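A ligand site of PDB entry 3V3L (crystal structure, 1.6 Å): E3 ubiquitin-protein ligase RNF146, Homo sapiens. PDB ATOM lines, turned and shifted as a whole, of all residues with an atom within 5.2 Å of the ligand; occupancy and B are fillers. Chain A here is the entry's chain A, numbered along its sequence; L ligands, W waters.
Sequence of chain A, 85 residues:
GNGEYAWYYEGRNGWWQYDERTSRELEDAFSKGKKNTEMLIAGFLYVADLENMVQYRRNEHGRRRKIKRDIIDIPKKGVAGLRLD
OH of Tyr 46 sits at hydrogen-bond distance from O5 of the ligand, at 2.5 Å.
The side-chain amino group (NZ) of Lys 77 lies within salt-bridge range of an oxygen (O2) of the ligand, at 2.7 Å.
NE of Arg 65 lies within salt-bridge range of O9 of the ligand (2.7 Å).
OH of Tyr 9 is in hydrogen-bond range of O3 of the ligand (2.7 Å).
O2 of the ligand lies within hydrogen-bond range of NE1 of Trp 16 (2.8 Å).
An oxygen (O6) of the ligand sits at hydrogen-bond distance from the backbone NH (N) of Arg 12 (2.9 Å).
NE of Arg 12 lies within salt-bridge range of O6 of the ligand (2.8 Å).
The side-chain amide nitrogen (NE2) of Gln 55 sits at hydrogen-bond distance from a nitrogen (N4) of the ligand, 2.9 Å away.
An oxygen (O1) of the ligand is in hydrogen-bond range of the backbone NH (N) of Arg 63 (3.1 Å).
O3 of the ligand lies close to N of Gly 81, 3.4 Å away.
N of Tyr 46 is in hydrogen-bond range of O of Met 39 (2.8 Å).
NZ of Lys 77 is in hydrogen-bond range of OD1 of Asn 13 (2.7 Å).
N of Gln 55 is in hydrogen-bond range of O of Arg 65.
The backbone carbonyl oxygen of Trp 16 lies within hydrogen-bond range of the backbone NH of Tyr 9 (2.8 Å).
The side-chain hydroxyl of Tyr 9 lies within hydrogen-bond range of the backbone NH of Gly 81.
OE1 of Gln 55 lies within hydrogen-bond range of OH of Tyr 18, 2.6 Å away.
CA of Gly 11 touches O2 of the ligand (3.6 Å).
CE2 of Tyr 18 touches N3 of the ligand (3.2 Å).
Ile 41 touches the ligand.
Gly 62 touches the ligand (CA to O1, 3.9 Å).
Ala 80 touches the ligand (CA to C1, 3.9 Å).
Hydrophobic or aromatic side chains that line the ligand: Tyr 9, Trp 16, Tyr 18, Ile 41 and Tyr 46.
Of the 19 residues printed, 14 come within 4 Å of the ligand.
The nearest printed residue that does not touch the ligand is Asn 13 (4.1 Å).
Water W1 lies within hydrogen-bond range of O10 of the ligand (2.5 Å) and NH2 of Arg 83 (3.0 Å).
Water W10 lies within hydrogen-bond range of an oxygen (O6) of the ligand and the guanidinium group (NH1) of Arg 65.
Water W4 lies within hydrogen-bond range of O1 of the ligand (2.7 Å) and NH2 of Arg 65 (3.1 Å).
Water W2 bridges OD1 of Asp 19 (2.7 Å) and N1 of the ligand (2.8 Å).
Water W8 lies within hydrogen-bond range of NZ of Lys 77, NH2 of Arg 83 and O10 of the ligand.
Water W6 lies within hydrogen-bond range of the backbone carbonyl oxygen of Arg 63, the backbone NH of Arg 57 and an oxygen (O5) of the ligand.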
ATOM      1  N   TYR A   9     -35.437  22.831 -20.907  1.00  0.00           N
ATOM      2  CA  TYR A   9     -34.188  23.093 -21.623  1.00  0.00           C
ATOM      3  C   TYR A   9     -33.234  21.899 -21.473  1.00  0.00           C
ATOM      4  O   TYR A   9     -33.232  21.218 -20.460  1.00  0.00           O
ATOM      5  CB  TYR A   9     -33.529  24.405 -21.188  1.00  0.00           C
ATOM      6  CG  TYR A   9     -33.110  24.453 -19.745  1.00  0.00           C
ATOM      7  CD1 TYR A   9     -34.006  24.849 -18.749  1.00  0.00           C
ATOM      8  CD2 TYR A   9     -31.819  24.092 -19.349  1.00  0.00           C
ATOM      9  CE1 TYR A   9     -33.657  24.852 -17.431  1.00  0.00           C
ATOM     10  CE2 TYR A   9     -31.440  24.122 -18.000  1.00  0.00           C
ATOM     11  CZ  TYR A   9     -32.366  24.495 -17.063  1.00  0.00           C
ATOM     12  OH  TYR A   9     -32.018  24.480 -15.760  1.00  0.00           O
ATOM     13  N   GLY A  11     -30.083  19.569 -20.909  1.00  0.00           N
ATOM     14  CA  GLY A  11     -28.801  19.316 -20.249  1.00  0.00           C
ATOM     15  C   GLY A  11     -28.010  18.302 -21.047  1.00  0.00           C
ATOM     16  O   GLY A  11     -28.434  17.854 -22.118  1.00  0.00           O
ATOM     17  N   ARG A  12     -26.876  17.875 -20.517  1.00  0.00           N
ATOM     18  CA  ARG A  12     -25.997  16.964 -21.263  1.00  0.00           C
ATOM     19  C   ARG A  12     -26.593  15.593 -21.551  1.00  0.00           C
ATOM     20  O   ARG A  12     -26.214  14.950 -22.547  1.00  0.00           O
ATOM     21  CB  ARG A  12     -24.642  16.827 -20.563  1.00  0.00           C
ATOM     22  CG  ARG A  12     -23.778  18.072 -20.738  1.00  0.00           C
ATOM     23  CD  ARG A  12     -22.562  18.131 -19.829  1.00  0.00           C
ATOM     24  NE  ARG A  12     -22.973  18.281 -18.429  1.00  0.00           N
ATOM     25  CZ  ARG A  12     -22.148  18.287 -17.396  1.00  0.00           C
ATOM     26  NH1 ARG A  12     -20.832  18.199 -17.573  1.00  0.00           N
ATOM     27  NH2 ARG A  12     -22.645  18.370 -16.179  1.00  0.00           N
ATOM     28  N   ASN A  13     -27.496  15.119 -20.692  1.00  0.00           N
ATOM     29  CA  ASN A  13     -28.063  13.780 -20.828  1.00  0.00           C
ATOM     30  C   ASN A  13     -29.532  13.700 -20.430  1.00  0.00           C
ATOM     31  O   ASN A  13     -30.025  12.646 -20.040  1.00  0.00           O
ATOM     32  CB  ASN A  13     -27.249  12.774 -20.006  1.00  0.00           C
ATOM     33  CG  ASN A  13     -27.301  13.072 -18.519  1.00  0.00           C
ATOM     34  OD1 ASN A  13     -27.714  14.163 -18.113  1.00  0.00           O
ATOM     35  ND2 ASN A  13     -26.870  12.100 -17.704  1.00  0.00           N
ATOM     36  N   TRP A  16     -34.096  19.625 -18.239  1.00  0.00           N
ATOM     37  CA  TRP A  16     -34.395  20.373 -17.033  1.00  0.00           C
ATOM     38  C   TRP A  16     -35.657  21.167 -17.269  1.00  0.00           C
ATOM     39  O   TRP A  16     -35.832  21.765 -18.327  1.00  0.00           O
ATOM     40  CB  TRP A  16     -33.276  21.367 -16.744  1.00  0.00           C
ATOM     41  CG  TRP A  16     -31.999  20.711 -16.328  1.00  0.00           C
ATOM     42  CD1 TRP A  16     -30.974  20.292 -17.140  1.00  0.00           C
ATOM     43  CD2 TRP A  16     -31.621  20.361 -14.997  1.00  0.00           C
ATOM     44  NE1 TRP A  16     -29.978  19.727 -16.385  1.00  0.00           N
ATOM     45  CE2 TRP A  16     -30.343  19.775 -15.064  1.00  0.00           C
ATOM     46  CE3 TRP A  16     -32.222  20.520 -13.745  1.00  0.00           C
ATOM     47  CZ2 TRP A  16     -29.670  19.316 -13.925  1.00  0.00           C
ATOM     48  CZ3 TRP A  16     -31.549  20.082 -12.617  1.00  0.00           C
ATOM     49  CH2 TRP A  16     -30.280  19.491 -12.720  1.00  0.00           C
ATOM     50  N   TYR A  18     -37.786  24.475 -16.843  1.00  0.00           N
ATOM     51  CA  TYR A  18     -37.599  25.882 -16.503  1.00  0.00           C
ATOM     52  C   TYR A  18     -38.239  26.233 -15.168  1.00  0.00           C
ATOM     53  O   TYR A  18     -39.270  25.669 -14.793  1.00  0.00           O
ATOM     54  CB  TYR A  18     -38.205  26.786 -17.568  1.00  0.00           C
ATOM     55  CG  TYR A  18     -37.361  27.005 -18.799  1.00  0.00           C
ATOM     56  CD1 TYR A  18     -37.505  26.200 -19.928  1.00  0.00           C
ATOM     57  CD2 TYR A  18     -36.434  28.042 -18.845  1.00  0.00           C
ATOM     58  CE1 TYR A  18     -36.749  26.417 -21.061  1.00  0.00           C
ATOM     59  CE2 TYR A  18     -35.685  28.290 -19.982  1.00  0.00           C
ATOM     60  CZ  TYR A  18     -35.849  27.481 -21.075  1.00  0.00           C
ATOM     61  OH  TYR A  18     -35.092  27.707 -22.194  1.00  0.00           O
ATOM     62  N   ASP A  19     -37.646  27.178 -14.455  1.00  0.00           N
ATOM     63  CA  ASP A  19     -38.286  27.761 -13.283  1.00  0.00           C
ATOM     64  C   ASP A  19     -39.674  28.319 -13.636  1.00  0.00           C
ATOM     65  O   ASP A  19     -39.938  28.666 -14.779  1.00  0.00           O
ATOM     66  CB  ASP A  19     -37.401  28.860 -12.693  1.00  0.00           C
ATOM     67  CG  ASP A  19     -37.388  30.125 -13.540  1.00  0.00           C
ATOM     68  OD1 ASP A  19     -36.493  30.268 -14.404  1.00  0.00           O
ATOM     69  OD2 ASP A  19     -38.248  31.002 -13.327  1.00  0.00           O
ATOM     70  N   MET A  39     -35.255  36.270 -21.517  1.00  0.00           N
ATOM     71  CA  MET A  39     -35.467  35.665 -20.214  1.00  0.00           C
ATOM     72  C   MET A  39     -34.293  36.110 -19.326  1.00  0.00           C
ATOM     73  O   MET A  39     -33.168  36.193 -19.809  1.00  0.00           O
ATOM     74  CB  MET A  39     -35.380  34.112 -20.292  1.00  0.00           C
ATOM     75  CG  MET A  39     -35.480  33.404 -21.710  1.00  0.00           C
ATOM     76  SD  MET A  39     -36.006  31.591 -21.372  1.00  0.00           S
ATOM     77  CE  MET A  39     -34.346  31.121 -22.219  1.00  0.00           C
ATOM     78  N   ILE A  41     -32.045  34.736 -16.368  1.00  0.00           N
ATOM     79  CA  ILE A  41     -31.671  33.473 -15.723  1.00  0.00           C
ATOM     80  C   ILE A  41     -30.483  33.723 -14.804  1.00  0.00           C
ATOM     81  O   ILE A  41     -29.407  34.028 -15.292  1.00  0.00           O
ATOM     82  CB  ILE A  41     -31.253  32.434 -16.786  1.00  0.00           C
ATOM     83  CG1 ILE A  41     -32.382  32.175 -17.788  1.00  0.00           C
ATOM     84  CG2 ILE A  41     -30.694  31.128 -16.126  1.00  0.00           C
ATOM     85  CD1 ILE A  41     -33.624  31.516 -17.208  1.00  0.00           C
ATOM     86  N   TYR A  46     -30.919  35.772 -21.403  1.00  0.00           N
ATOM     87  CA  TYR A  46     -30.946  34.743 -22.438  1.00  0.00           C
ATOM     88  C   TYR A  46     -32.018  35.061 -23.469  1.00  0.00           C
ATOM     89  O   TYR A  46     -33.023  35.696 -23.173  1.00  0.00           O
ATOM     90  CB  TYR A  46     -31.210  33.377 -21.820  1.00  0.00           C
ATOM     91  CG  TYR A  46     -30.000  32.744 -21.176  1.00  0.00           C
ATOM     92  CD1 TYR A  46     -29.479  33.237 -19.996  1.00  0.00           C
ATOM     93  CD2 TYR A  46     -29.370  31.634 -21.765  1.00  0.00           C
ATOM     94  CE1 TYR A  46     -28.328  32.663 -19.414  1.00  0.00           C
ATOM     95  CE2 TYR A  46     -28.240  31.039 -21.177  1.00  0.00           C
ATOM     96  CZ  TYR A  46     -27.719  31.574 -20.006  1.00  0.00           C
ATOM     97  OH  TYR A  46     -26.610  31.027 -19.404  1.00  0.00           O
ATOM     98  N   GLN A  55     -32.349  28.006 -26.824  1.00  0.00           N
ATOM     99  CA  GLN A  55     -31.978  29.162 -26.017  1.00  0.00           C
ATOM    100  C   GLN A  55     -30.463  29.343 -26.020  1.00  0.00           C
ATOM    101  O   GLN A  55     -29.702  28.394 -26.209  1.00  0.00           O
ATOM    102  CB  GLN A  55     -32.472  29.033 -24.563  1.00  0.00           C
ATOM    103  CG  GLN A  55     -31.878  27.880 -23.757  1.00  0.00           C
ATOM    104  CD  GLN A  55     -31.704  28.225 -22.259  1.00  0.00           C
ATOM    105  OE1 GLN A  55     -32.697  28.383 -21.531  1.00  0.00           O
ATOM    106  NE2 GLN A  55     -30.451  28.279 -21.795  1.00  0.00           N
ATOM    107  N   ARG A  57     -27.274  32.461 -24.459  1.00  0.00           N
ATOM    108  CA  ARG A  57     -27.042  33.700 -23.743  1.00  0.00           C
ATOM    109  C   ARG A  57     -27.030  34.855 -24.754  1.00  0.00           C
ATOM    110  O   ARG A  57     -26.521  34.707 -25.858  1.00  0.00           O
ATOM    111  CB  ARG A  57     -25.732  33.650 -22.938  1.00  0.00           C
ATOM    112  CG  ARG A  57     -25.654  34.846 -22.027  1.00  0.00           C
ATOM    113  CD  ARG A  57     -24.711  34.728 -20.900  1.00  0.00           C
ATOM    114  NE  ARG A  57     -24.439  36.053 -20.383  1.00  0.00           N
ATOM    115  CZ  ARG A  57     -23.385  36.375 -19.633  1.00  0.00           C
ATOM    116  NH1 ARG A  57     -22.493  35.449 -19.290  1.00  0.00           N
ATOM    117  NH2 ARG A  57     -23.230  37.622 -19.220  1.00  0.00           N
ATOM    118  N   GLY A  62     -21.909  31.117 -25.054  1.00  0.00           N
ATOM    119  CA  GLY A  62     -22.434  30.032 -24.247  1.00  0.00           C
ATOM    120  C   GLY A  62     -22.950  28.930 -25.154  1.00  0.00           C
ATOM    121  O   GLY A  62     -22.920  29.042 -26.368  1.00  0.00           O
ATOM    122  N   ARG A  63     -23.434  27.869 -24.538  1.00  0.00           N
ATOM    123  CA  ARG A  63     -24.040  26.772 -25.240  1.00  0.00           C
ATOM    124  C   ARG A  63     -25.345  27.191 -25.942  1.00  0.00           C
ATOM    125  O   ARG A  63     -26.045  28.084 -25.470  1.00  0.00           O
ATOM    126  CB  ARG A  63     -24.376  25.745 -24.184  1.00  0.00           C
ATOM    127  CG  ARG A  63     -24.618  24.413 -24.647  1.00  0.00           C
ATOM    128  CD  ARG A  63     -24.495  23.559 -23.462  1.00  0.00           C
ATOM    129  NE  ARG A  63     -25.095  22.273 -23.704  1.00  0.00           N
ATOM    130  CZ  ARG A  63     -24.648  21.144 -23.166  1.00  0.00           C
ATOM    131  NH1 ARG A  63     -23.571  21.145 -22.352  1.00  0.00           N
ATOM    132  NH2 ARG A  63     -25.291  20.022 -23.428  1.00  0.00           N
ATOM    133  N   ARG A  65     -28.787  25.549 -26.236  1.00  0.00           N
ATOM    134  CA  ARG A  65     -29.555  24.435 -25.671  1.00  0.00           C
ATOM    135  C   ARG A  65     -30.910  24.318 -26.346  1.00  0.00           C
ATOM    136  O   ARG A  65     -31.630  25.299 -26.497  1.00  0.00           O
ATOM    137  CB  ARG A  65     -29.792  24.622 -24.175  1.00  0.00           C
ATOM    138  CG  ARG A  65     -28.523  24.581 -23.352  1.00  0.00           C
ATOM    139  CD  ARG A  65     -28.777  24.949 -21.932  1.00  0.00           C
ATOM    140  NE  ARG A  65     -27.534  25.071 -21.209  1.00  0.00           N
ATOM    141  CZ  ARG A  65     -26.918  24.098 -20.553  1.00  0.00           C
ATOM    142  NH1 ARG A  65     -27.460  22.909 -20.443  1.00  0.00           N
ATOM    143  NH2 ARG A  65     -25.752  24.337 -19.955  1.00  0.00           N
ATOM    144  N   LYS A  77     -34.580  15.984 -15.051  1.00  0.00           N
ATOM    145  CA  LYS A  77     -33.462  16.029 -14.111  1.00  0.00           C
ATOM    146  C   LYS A  77     -33.731  16.885 -12.878  1.00  0.00           C
ATOM    147  O   LYS A  77     -33.105  16.714 -11.872  1.00  0.00           O
ATOM    148  CB  LYS A  77     -32.212  16.541 -14.809  1.00  0.00           C
ATOM    149  CG  LYS A  77     -31.725  15.619 -15.917  1.00  0.00           C
ATOM    150  CD  LYS A  77     -30.352  15.964 -16.413  1.00  0.00           C
ATOM    151  CE  LYS A  77     -29.287  15.605 -15.379  1.00  0.00           C
ATOM    152  NZ  LYS A  77     -27.916  15.710 -15.891  1.00  0.00           N
ATOM    153  N   ALA A  80     -34.574  24.054 -13.102  1.00  0.00           N
ATOM    154  CA  ALA A  80     -33.686  25.224 -13.074  1.00  0.00           C
ATOM    155  C   ALA A  80     -32.345  24.924 -12.366  1.00  0.00           C
ATOM    156  O   ALA A  80     -31.809  25.768 -11.649  1.00  0.00           O
ATOM    157  CB  ALA A  80     -34.406  26.418 -12.435  1.00  0.00           C
ATOM    158  N   GLY A  81     -31.832  23.716 -12.569  1.00  0.00           N
ATOM    159  CA  GLY A  81     -30.553  23.320 -11.970  1.00  0.00           C
ATOM    160  C   GLY A  81     -30.640  22.693 -10.582  1.00  0.00           C
ATOM    161  O   GLY A  81     -29.626  22.237 -10.057  1.00  0.00           O
ATOM    162  N   ARG A  83     -31.627  19.670  -8.685  1.00  0.00           N
ATOM    163  CA  ARG A  83     -31.867  18.264  -8.951  1.00  0.00           C
ATOM    164  C   ARG A  83     -33.140  17.776  -8.284  1.00  0.00           C
ATOM    165  O   ARG A  83     -33.436  18.181  -7.157  1.00  0.00           O
ATOM    166  CB  ARG A  83     -30.685  17.426  -8.439  1.00  0.00           C
ATOM    167  CG  ARG A  83     -29.494  17.462  -9.358  1.00  0.00           C
ATOM    168  CD  ARG A  83     -29.806  16.682 -10.597  1.00  0.00           C
ATOM    169  NE  ARG A  83     -28.688  16.611 -11.541  1.00  0.00           N
ATOM    170  CZ  ARG A  83     -27.962  15.522 -11.739  1.00  0.00           C
ATOM    171  NH1 ARG A  83     -28.231  14.402 -11.069  1.00  0.00           N
ATOM    172  NH2 ARG A  83     -26.975  15.545 -12.615  1.00  0.00           N
HETATM  173  N1  LIG L   1     -32.366  27.825 -16.216  1.00  0.00           N
HETATM  174  C1  LIG L   1     -31.445  27.596 -15.245  1.00  0.00           C
HETATM  175  N2  LIG L   1     -30.125  27.546 -15.482  1.00  0.00           N
HETATM  176  C2  LIG L   1     -29.636  27.710 -16.731  1.00  0.00           C
HETATM  177  C3  LIG L   1     -30.564  27.946 -17.844  1.00  0.00           C
HETATM  178  C4  LIG L   1     -31.993  27.966 -17.521  1.00  0.00           C
HETATM  179  N3  LIG L   1     -32.859  28.177 -18.511  1.00  0.00           N
HETATM  180  N4  LIG L   1     -29.829  28.072 -18.967  1.00  0.00           N
HETATM  181  C5  LIG L   1     -28.553  27.918 -18.616  1.00  0.00           C
HETATM  182  N5  LIG L   1     -28.437  27.731 -17.289  1.00  0.00           N
HETATM  183  P1  LIG L   1     -25.082  28.079 -21.063  1.00  0.00           P
HETATM  184  P2  LIG L   1     -26.384  18.753 -16.861  1.00  0.00           P
HETATM  185  C6  LIG L   1     -27.606  23.813 -16.635  1.00  0.00           C
HETATM  186  C7  LIG L   1     -27.167  27.463 -16.588  1.00  0.00           C
HETATM  187  O1  LIG L   1     -23.715  27.581 -21.501  1.00  0.00           O
HETATM  188  O2  LIG L   1     -27.731  18.131 -17.043  1.00  0.00           O
HETATM  189  C8  LIG L   1     -28.475  23.030 -15.645  1.00  0.00           C
HETATM  190  O3  LIG L   1     -29.452  23.858 -15.041  1.00  0.00           O
HETATM  191  C9  LIG L   1     -26.720  26.050 -17.000  1.00  0.00           C
HETATM  192  O4  LIG L   1     -27.311  25.105 -16.100  1.00  0.00           O
HETATM  193  O5  LIG L   1     -25.224  29.591 -20.974  1.00  0.00           O
HETATM  194  O6  LIG L   1     -25.700  19.034 -18.177  1.00  0.00           O
HETATM  195  C10 LIG L   1     -27.468  22.485 -14.646  1.00  0.00           C
HETATM  196  O7  LIG L   1     -27.302  23.338 -13.505  1.00  0.00           O
HETATM  197  C11 LIG L   1     -25.189  26.145 -16.957  1.00  0.00           C
HETATM  198  O8  LIG L   1     -24.618  25.695 -15.733  1.00  0.00           O
HETATM  199  O9  LIG L   1     -26.218  27.368 -21.757  1.00  0.00           O
HETATM  200  O10 LIG L   1     -25.476  18.097 -15.858  1.00  0.00           O
HETATM  201  C12 LIG L   1     -26.166  22.423 -15.433  1.00  0.00           C
HETATM  202  O11 LIG L   1     -26.392  23.057 -16.698  1.00  0.00           O
HETATM  203  C13 LIG L   1     -24.891  27.628 -17.148  1.00  0.00           C
HETATM  204  O12 LIG L   1     -26.129  28.332 -16.989  1.00  0.00           O
HETATM  205  C14 LIG L   1     -25.668  21.005 -15.648  1.00  0.00           C
HETATM  206  O13 LIG L   1     -26.691  20.172 -16.184  1.00  0.00           O
HETATM  207  C15 LIG L   1     -24.351  27.997 -18.516  1.00  0.00           C
HETATM  208  O14 LIG L   1     -25.227  27.531 -19.570  1.00  0.00           O
HETATM  209  O   HOH W   1     -25.506  18.051 -13.394  1.00  0.00           O
HETATM  210  O   HOH W   2     -35.060  28.233 -15.537  1.00  0.00           O
HETATM  211  O   HOH W   3     -28.170  28.039 -23.462  1.00  0.00           O
HETATM  212  O   HOH W   4     -22.861  25.329 -20.231  1.00  0.00           O
HETATM  213  O   HOH W   5     -26.041  25.945 -13.384  1.00  0.00           O
HETATM  214  O   HOH W   6     -25.634  30.280 -23.793  1.00  0.00           O
HETATM  215  O   HOH W   7     -28.994  26.030 -13.419  1.00  0.00           O
HETATM  216  O   HOH W   8     -25.413  15.310 -15.012  1.00  0.00           O
HETATM  217  O   HOH W   9     -27.353  21.708 -11.275  1.00  0.00           O
HETATM  218  O   HOH W  10     -25.401  21.524 -19.161  1.00  0.00           O
